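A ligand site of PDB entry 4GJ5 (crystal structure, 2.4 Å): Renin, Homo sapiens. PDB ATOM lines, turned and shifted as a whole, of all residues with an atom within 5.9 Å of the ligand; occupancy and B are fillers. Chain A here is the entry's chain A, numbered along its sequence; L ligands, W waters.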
ATOM      1  N   THR A  18     -13.044  -2.851  -0.110  1.00  0.00           N
ATOM      2  CA  THR A  18     -12.884  -2.148  -1.390  1.00  0.00           C
ATOM      3  C   THR A  18     -14.169  -1.564  -1.937  1.00  0.00           C
ATOM      4  O   THR A  18     -14.114  -0.611  -2.722  1.00  0.00           O
ATOM      5  CB  THR A  18     -12.186  -3.015  -2.424  1.00  0.00           C
ATOM      6  OG1 THR A  18     -12.905  -4.234  -2.587  1.00  0.00           O
ATOM      7  CG2 THR A  18     -10.741  -3.293  -2.055  1.00  0.00           C
ATOM      8  N   GLN A  19     -15.328  -2.125  -1.567  1.00  0.00           N
ATOM      9  CA  GLN A  19     -16.603  -1.618  -2.068  1.00  0.00           C
ATOM     10  C   GLN A  19     -17.587  -1.442  -0.936  1.00  0.00           C
ATOM     11  O   GLN A  19     -17.863  -2.409  -0.235  1.00  0.00           O
ATOM     12  CB  GLN A  19     -17.188  -2.547  -3.158  1.00  0.00           C
ATOM     13  CG  GLN A  19     -16.237  -2.857  -4.330  1.00  0.00           C
ATOM     14  CD  GLN A  19     -16.830  -3.893  -5.252  1.00  0.00           C
ATOM     15  OE1 GLN A  19     -18.037  -3.921  -5.523  1.00  0.00           O
ATOM     16  NE2 GLN A  19     -15.972  -4.736  -5.809  1.00  0.00           N
ATOM     17  N   VAL A  36     -22.934   2.648  -4.875  1.00  0.00           N
ATOM     18  CA  VAL A  36     -21.783   3.266  -4.235  1.00  0.00           C
ATOM     19  C   VAL A  36     -22.124   4.758  -4.190  1.00  0.00           C
ATOM     20  O   VAL A  36     -22.599   5.318  -5.194  1.00  0.00           O
ATOM     21  CB  VAL A  36     -20.463   2.934  -4.993  1.00  0.00           C
ATOM     22  CG1 VAL A  36     -19.352   3.933  -4.632  1.00  0.00           C
ATOM     23  CG2 VAL A  36     -20.002   1.522  -4.646  1.00  0.00           C
ATOM     24  N   ASP A  38     -20.723   8.072  -4.201  1.00  0.00           N
ATOM     25  CA  ASP A  38     -19.436   8.577  -4.639  1.00  0.00           C
ATOM     26  C   ASP A  38     -19.280  10.084  -4.716  1.00  0.00           C
ATOM     27  O   ASP A  38     -19.852  10.704  -5.613  1.00  0.00           O
ATOM     28  CB  ASP A  38     -19.083   7.862  -5.948  1.00  0.00           C
ATOM     29  CG  ASP A  38     -17.853   8.315  -6.682  1.00  0.00           C
ATOM     30  OD1 ASP A  38     -16.835   8.605  -6.024  1.00  0.00           O
ATOM     31  OD2 ASP A  38     -17.881   8.312  -7.925  1.00  0.00           O
ATOM     32  N   GLY A  40     -16.573  11.573  -5.733  1.00  0.00           N
ATOM     33  CA  GLY A  40     -15.746  11.785  -6.921  1.00  0.00           C
ATOM     34  C   GLY A  40     -16.504  11.844  -8.242  1.00  0.00           C
ATOM     35  O   GLY A  40     -15.905  11.978  -9.299  1.00  0.00           O
ATOM     36  N   SER A  41     -17.836  11.699  -8.211  1.00  0.00           N
ATOM     37  CA  SER A  41     -18.701  11.808  -9.414  1.00  0.00           C
ATOM     38  C   SER A  41     -20.015  12.541  -9.058  1.00  0.00           C
ATOM     39  O   SER A  41     -20.307  12.684  -7.869  1.00  0.00           O
ATOM     40  CB  SER A  41     -18.952  10.447 -10.068  1.00  0.00           C
ATOM     41  OG  SER A  41     -19.795   9.601  -9.303  1.00  0.00           O
ATOM     42  N   TRP A  45     -26.624   6.820 -11.747  1.00  0.00           N
ATOM     43  CA  TRP A  45     -26.819   5.839 -12.812  1.00  0.00           C
ATOM     44  C   TRP A  45     -27.024   4.450 -12.241  1.00  0.00           C
ATOM     45  O   TRP A  45     -26.446   4.101 -11.215  1.00  0.00           O
ATOM     46  CB  TRP A  45     -25.722   5.865 -13.902  1.00  0.00           C
ATOM     47  CG  TRP A  45     -24.379   5.343 -13.462  1.00  0.00           C
ATOM     48  CD1 TRP A  45     -23.329   6.079 -12.999  1.00  0.00           C
ATOM     49  CD2 TRP A  45     -23.945   3.975 -13.458  1.00  0.00           C
ATOM     50  NE1 TRP A  45     -22.263   5.257 -12.721  1.00  0.00           N
ATOM     51  CE2 TRP A  45     -22.624   3.958 -12.966  1.00  0.00           C
ATOM     52  CE3 TRP A  45     -24.558   2.742 -13.793  1.00  0.00           C
ATOM     53  CZ2 TRP A  45     -21.875   2.777 -12.833  1.00  0.00           C
ATOM     54  CZ3 TRP A  45     -23.828   1.563 -13.640  1.00  0.00           C
ATOM     55  CH2 TRP A  45     -22.517   1.587 -13.140  1.00  0.00           C
ATOM     56  N   LEU A  81     -20.323   8.558 -19.183  1.00  0.00           N
ATOM     57  CA  LEU A  81     -19.602   8.884 -17.960  1.00  0.00           C
ATOM     58  C   LEU A  81     -18.242   8.212 -18.040  1.00  0.00           C
ATOM     59  O   LEU A  81     -18.156   6.988 -18.030  1.00  0.00           O
ATOM     60  CB  LEU A  81     -20.401   8.445 -16.715  1.00  0.00           C
ATOM     61  CG  LEU A  81     -21.885   8.875 -16.664  1.00  0.00           C
ATOM     62  CD1 LEU A  81     -22.618   8.197 -15.523  1.00  0.00           C
ATOM     63  CD2 LEU A  81     -22.043  10.383 -16.513  1.00  0.00           C
ATOM     64  N   TYR A  83     -14.392   7.835 -16.524  1.00  0.00           N
ATOM     65  CA  TYR A  83     -13.495   7.972 -15.381  1.00  0.00           C
ATOM     66  C   TYR A  83     -12.289   7.067 -15.511  1.00  0.00           C
ATOM     67  O   TYR A  83     -12.267   6.163 -16.326  1.00  0.00           O
ATOM     68  CB  TYR A  83     -14.229   7.720 -14.041  1.00  0.00           C
ATOM     69  CG  TYR A  83     -15.291   8.756 -13.755  1.00  0.00           C
ATOM     70  CD1 TYR A  83     -14.945  10.014 -13.245  1.00  0.00           C
ATOM     71  CD2 TYR A  83     -16.630   8.490 -14.005  1.00  0.00           C
ATOM     72  CE1 TYR A  83     -15.908  10.977 -12.985  1.00  0.00           C
ATOM     73  CE2 TYR A  83     -17.613   9.442 -13.754  1.00  0.00           C
ATOM     74  CZ  TYR A  83     -17.238  10.689 -13.264  1.00  0.00           C
ATOM     75  OH  TYR A  83     -18.192  11.637 -13.054  1.00  0.00           O
ATOM     76  N   THR A  85     -11.380   4.848 -13.428  1.00  0.00           N
ATOM     77  CA  THR A  85     -11.826   3.523 -12.977  1.00  0.00           C
ATOM     78  C   THR A  85     -12.600   2.785 -14.087  1.00  0.00           C
ATOM     79  O   THR A  85     -12.536   1.564 -14.177  1.00  0.00           O
ATOM     80  CB  THR A  85     -12.637   3.670 -11.675  1.00  0.00           C
ATOM     81  OG1 THR A  85     -11.837   4.328 -10.700  1.00  0.00           O
ATOM     82  CG2 THR A  85     -13.120   2.335 -11.102  1.00  0.00           C
ATOM     83  N   GLY A  86     -13.358   3.525 -14.888  1.00  0.00           N
ATOM     84  CA  GLY A  86     -14.178   2.933 -15.928  1.00  0.00           C
ATOM     85  C   GLY A  86     -15.132   3.885 -16.610  1.00  0.00           C
ATOM     86  O   GLY A  86     -15.270   5.049 -16.224  1.00  0.00           O
ATOM     87  N   THR A  87     -15.762   3.379 -17.681  1.00  0.00           N
ATOM     88  CA  THR A  87     -16.681   4.136 -18.530  1.00  0.00           C
ATOM     89  C   THR A  87     -18.005   3.393 -18.725  1.00  0.00           C
ATOM     90  O   THR A  87     -18.008   2.247 -19.170  1.00  0.00           O
ATOM     91  CB  THR A  87     -15.996   4.489 -19.866  1.00  0.00           C
ATOM     92  OG1 THR A  87     -14.830   5.251 -19.579  1.00  0.00           O
ATOM     93  CG2 THR A  87     -16.908   5.278 -20.838  1.00  0.00           C
ATOM     94  N   VAL A  88     -19.121   4.078 -18.451  1.00  0.00           N
ATOM     95  CA  VAL A  88     -20.453   3.563 -18.682  1.00  0.00           C
ATOM     96  C   VAL A  88     -21.123   4.477 -19.679  1.00  0.00           C
ATOM     97  O   VAL A  88     -20.791   5.661 -19.766  1.00  0.00           O
ATOM     98  CB  VAL A  88     -21.327   3.368 -17.404  1.00  0.00           C
ATOM     99  CG1 VAL A  88     -20.771   2.266 -16.511  1.00  0.00           C
ATOM    100  CG2 VAL A  88     -21.535   4.682 -16.636  1.00  0.00           C
ATOM    101  N   PRO A 118     -14.183  -2.630 -15.358  1.00  0.00           N
ATOM    102  CA  PRO A 118     -14.144  -3.345 -14.071  1.00  0.00           C
ATOM    103  C   PRO A 118     -15.488  -3.820 -13.503  1.00  0.00           C
ATOM    104  O   PRO A 118     -15.510  -4.326 -12.381  1.00  0.00           O
ATOM    105  CB  PRO A 118     -13.521  -2.280 -13.162  1.00  0.00           C
ATOM    106  CG  PRO A 118     -14.206  -1.004 -13.624  1.00  0.00           C
ATOM    107  CD  PRO A 118     -14.421  -1.186 -15.130  1.00  0.00           C
ATOM    108  N   PHE A 119     -16.613  -3.665 -14.262  1.00  0.00           N
ATOM    109  CA  PHE A 119     -17.987  -3.946 -13.798  1.00  0.00           C
ATOM    110  C   PHE A 119     -18.367  -5.401 -13.459  1.00  0.00           C
ATOM    111  O   PHE A 119     -19.375  -5.600 -12.789  1.00  0.00           O
ATOM    112  CB  PHE A 119     -19.054  -3.151 -14.576  1.00  0.00           C
ATOM    113  CG  PHE A 119     -18.814  -1.653 -14.494  1.00  0.00           C
ATOM    114  CD1 PHE A 119     -19.171  -0.942 -13.356  1.00  0.00           C
ATOM    115  CD2 PHE A 119     -18.158  -0.986 -15.522  1.00  0.00           C
ATOM    116  CE1 PHE A 119     -18.912   0.427 -13.255  1.00  0.00           C
ATOM    117  CE2 PHE A 119     -17.889   0.393 -15.422  1.00  0.00           C
ATOM    118  CZ  PHE A 119     -18.256   1.095 -14.283  1.00  0.00           C
ATOM    119  N   LEU A 121     -16.305  -7.091 -11.522  1.00  0.00           N
ATOM    120  CA  LEU A 121     -15.765  -7.085 -10.171  1.00  0.00           C
ATOM    121  C   LEU A 121     -16.655  -6.348  -9.173  1.00  0.00           C
ATOM    122  O   LEU A 121     -16.460  -6.500  -7.972  1.00  0.00           O
ATOM    123  CB  LEU A 121     -14.348  -6.479 -10.189  1.00  0.00           C
ATOM    124  CG  LEU A 121     -13.336  -7.144 -11.144  1.00  0.00           C
ATOM    125  CD1 LEU A 121     -12.141  -6.224 -11.421  1.00  0.00           C
ATOM    126  CD2 LEU A 121     -12.882  -8.534 -10.638  1.00  0.00           C
ATOM    127  N   ALA A 122     -17.627  -5.555  -9.692  1.00  0.00           N
ATOM    128  CA  ALA A 122     -18.560  -4.761  -8.879  1.00  0.00           C
ATOM    129  C   ALA A 122     -19.687  -5.587  -8.279  1.00  0.00           C
ATOM    130  O   ALA A 122     -20.431  -6.255  -9.004  1.00  0.00           O
ATOM    131  CB  ALA A 122     -19.134  -3.634  -9.703  1.00  0.00           C
ATOM    132  N   PHE A 124     -22.020  -4.069  -6.445  1.00  0.00           N
ATOM    133  CA  PHE A 124     -23.099  -3.098  -6.484  1.00  0.00           C
ATOM    134  C   PHE A 124     -23.599  -2.991  -7.925  1.00  0.00           C
ATOM    135  O   PHE A 124     -22.924  -3.459  -8.838  1.00  0.00           O
ATOM    136  CB  PHE A 124     -22.601  -1.730  -5.966  1.00  0.00           C
ATOM    137  CG  PHE A 124     -21.400  -1.198  -6.716  1.00  0.00           C
ATOM    138  CD1 PHE A 124     -20.106  -1.542  -6.318  1.00  0.00           C
ATOM    139  CD2 PHE A 124     -21.554  -0.367  -7.818  1.00  0.00           C
ATOM    140  CE1 PHE A 124     -18.995  -1.065  -7.011  1.00  0.00           C
ATOM    141  CE2 PHE A 124     -20.444   0.110  -8.521  1.00  0.00           C
ATOM    142  CZ  PHE A 124     -19.169  -0.244  -8.112  1.00  0.00           C
ATOM    143  N   VAL A 127     -24.166   3.785  -9.236  1.00  0.00           N
ATOM    144  CA  VAL A 127     -23.417   4.825  -8.509  1.00  0.00           C
ATOM    145  C   VAL A 127     -24.338   6.006  -8.276  1.00  0.00           C
ATOM    146  O   VAL A 127     -25.054   6.405  -9.203  1.00  0.00           O
ATOM    147  CB  VAL A 127     -22.088   5.217  -9.241  1.00  0.00           C
ATOM    148  CG1 VAL A 127     -21.389   6.422  -8.595  1.00  0.00           C
ATOM    149  CG2 VAL A 127     -21.124   4.018  -9.323  1.00  0.00           C
ATOM    150  N   LEU A 224      -8.297  14.960  -3.307  1.00  0.00           N
ATOM    151  CA  LEU A 224      -9.706  14.724  -3.568  1.00  0.00           C
ATOM    152  C   LEU A 224     -10.164  13.727  -2.490  1.00  0.00           C
ATOM    153  O   LEU A 224      -9.481  12.736  -2.240  1.00  0.00           O
ATOM    154  CB  LEU A 224      -9.874  14.099  -4.962  1.00  0.00           C
ATOM    155  CG  LEU A 224     -11.297  13.838  -5.421  1.00  0.00           C
ATOM    156  CD1 LEU A 224     -12.029  15.154  -5.765  1.00  0.00           C
ATOM    157  CD2 LEU A 224     -11.314  12.838  -6.579  1.00  0.00           C
ATOM    158  N   ASP A 226     -12.574  11.118  -1.917  1.00  0.00           N
ATOM    159  CA  ASP A 226     -13.365  10.265  -2.828  1.00  0.00           C
ATOM    160  C   ASP A 226     -13.916   9.025  -2.190  1.00  0.00           C
ATOM    161  O   ASP A 226     -13.236   8.013  -2.089  1.00  0.00           O
ATOM    162  CB  ASP A 226     -12.526   9.930  -4.085  1.00  0.00           C
ATOM    163  CG  ASP A 226     -13.279   9.297  -5.264  1.00  0.00           C
ATOM    164  OD1 ASP A 226     -14.480   8.971  -5.102  1.00  0.00           O
ATOM    165  OD2 ASP A 226     -12.664   9.159  -6.351  1.00  0.00           O
ATOM    166  N   GLY A 228     -16.088   6.845  -3.341  1.00  0.00           N
ATOM    167  CA  GLY A 228     -16.212   5.741  -4.288  1.00  0.00           C
ATOM    168  C   GLY A 228     -14.908   5.040  -4.635  1.00  0.00           C
ATOM    169  O   GLY A 228     -14.932   3.937  -5.153  1.00  0.00           O
ATOM    170  N   ALA A 229     -13.753   5.683  -4.319  1.00  0.00           N
ATOM    171  CA  ALA A 229     -12.434   5.101  -4.536  1.00  0.00           C
ATOM    172  C   ALA A 229     -12.070   4.143  -3.368  1.00  0.00           C
ATOM    173  O   ALA A 229     -12.261   4.484  -2.196  1.00  0.00           O
ATOM    174  CB  ALA A 229     -11.394   6.203  -4.682  1.00  0.00           C
ATOM    175  N   SER A 230     -11.632   2.930  -3.698  1.00  0.00           N
ATOM    176  CA  SER A 230     -11.283   1.886  -2.734  1.00  0.00           C
ATOM    177  C   SER A 230     -10.032   2.215  -1.925  1.00  0.00           C
ATOM    178  O   SER A 230      -9.921   1.860  -0.767  1.00  0.00           O
ATOM    179  CB  SER A 230     -11.015   0.565  -3.453  1.00  0.00           C
ATOM    180  OG  SER A 230     -12.098   0.154  -4.260  1.00  0.00           O
HETATM  181  C1  LIG L   1     -19.009   6.284 -12.210  1.00  0.00           C
HETATM  182  C2  LIG L   1     -18.053   6.678 -11.248  1.00  0.00           C
HETATM  183  C3  LIG L   1     -16.739   6.150 -11.278  1.00  0.00           C
HETATM  184  C4  LIG L   1     -16.383   5.236 -12.311  1.00  0.00           C
HETATM  185  C5  LIG L   1     -17.339   4.832 -13.272  1.00  0.00           C
HETATM  186  C6  LIG L   1     -18.642   5.361 -13.222  1.00  0.00           C
HETATM  187  C7  LIG L   1     -15.652   6.634 -10.306  1.00  0.00           C
HETATM  188  C8  LIG L   1     -15.719   6.000  -8.882  1.00  0.00           C
HETATM  189  C9  LIG L   1     -14.554   8.745  -9.287  1.00  0.00           C
HETATM  190  C10 LIG L   1     -15.602   8.209 -10.286  1.00  0.00           C
HETATM  191  N1  LIG L   1     -14.724   8.033  -7.995  1.00  0.00           N
HETATM  192  C11 LIG L   1     -14.563   6.554  -8.028  1.00  0.00           C
HETATM  193  O1  LIG L   1     -15.629   4.583  -9.038  1.00  0.00           O
HETATM  194  C12 LIG L   1     -16.695   3.838  -8.436  1.00  0.00           C
HETATM  195  C13 LIG L   1     -16.433   2.397  -8.885  1.00  0.00           C
HETATM  196  C14 LIG L   1     -16.766   2.020 -10.203  1.00  0.00           C
HETATM  197  C15 LIG L   1     -16.542   0.719 -10.662  1.00  0.00           C
HETATM  198  C16 LIG L   1     -15.845   1.454  -8.015  1.00  0.00           C
HETATM  199  C17 LIG L   1     -15.631   0.133  -8.472  1.00  0.00           C
HETATM  200  C18 LIG L   1     -16.014  -0.243  -9.789  1.00  0.00           C
HETATM  201  C19 LIG L   1     -15.840  -1.563 -10.245  1.00  0.00           C
HETATM  202  C20 LIG L   1     -15.253  -2.510  -9.414  1.00  0.00           C
HETATM  203  C21 LIG L   1     -14.840  -2.135  -8.118  1.00  0.00           C
HETATM  204  C22 LIG L   1     -15.044  -0.832  -7.630  1.00  0.00           C
HETATM  205  O   HOH W   1     -11.807  10.841  -9.708  1.00  0.00           O
HETATM  206  O   HOH W   2     -11.258   6.293  -8.634  1.00  0.00           O
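The side-chain carboxylate (OD2) of Asp 226 is in salt-bridge range of a nitrogen (N1) of the ligand (2.9 Å). The side-chain carboxylate (OD1) of Asp 38 lies within salt-bridge range of a nitrogen (N1) of the ligand.
Merely in contact with the ligand: Gln 19, Gly 40, Ser 41, Trp 45, Tyr 83, Thr 85, Gly 86, Pro 118, Phe 119, Ala 122, Phe 124, Gly 228 and Ala 229. Hydrophobic or aromatic side chains within 4 Å of the ligand: Tyr 83, Pro 118, Phe 119, Ala 122 and Phe 124. Of the 24 residues printed, 15 come within 4 Å of the ligand.
The side-chain carboxylate (OD1) of Asp 226 sits close to the side-chain carboxylate (OD1) of Asp 38. The side-chain carboxylate (OD1) of Asp 226 sits at hydrogen-bond distance from the backbone NH (N) of Gly 40. The side-chain carboxylate (OD1) of Asp 226 sits at hydrogen-bond distance from the backbone NH (N) of Gly 228 (3.2 Å). The side-chain carboxylate of Asp 226 is in hydrogen-bond range of the backbone NH of Ala 229. OD1 of Asp 38 lies within hydrogen-bond range of N of Gly 40 (3.0 Å). N of Gly 228 sits at hydrogen-bond distance from OD1 of Asp 38, at 3.3 Å. The side-chain carboxylate (OD2) of Asp 38 is in hydrogen-bond range of the side-chain hydroxyl (OG) of Ser 41, at 2.7 Å. The backbone carbonyl oxygen (O) of Leu 121 is in hydrogen-bond range of the side-chain amide nitrogen (NE2) of Gln 19 (2.8 Å).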
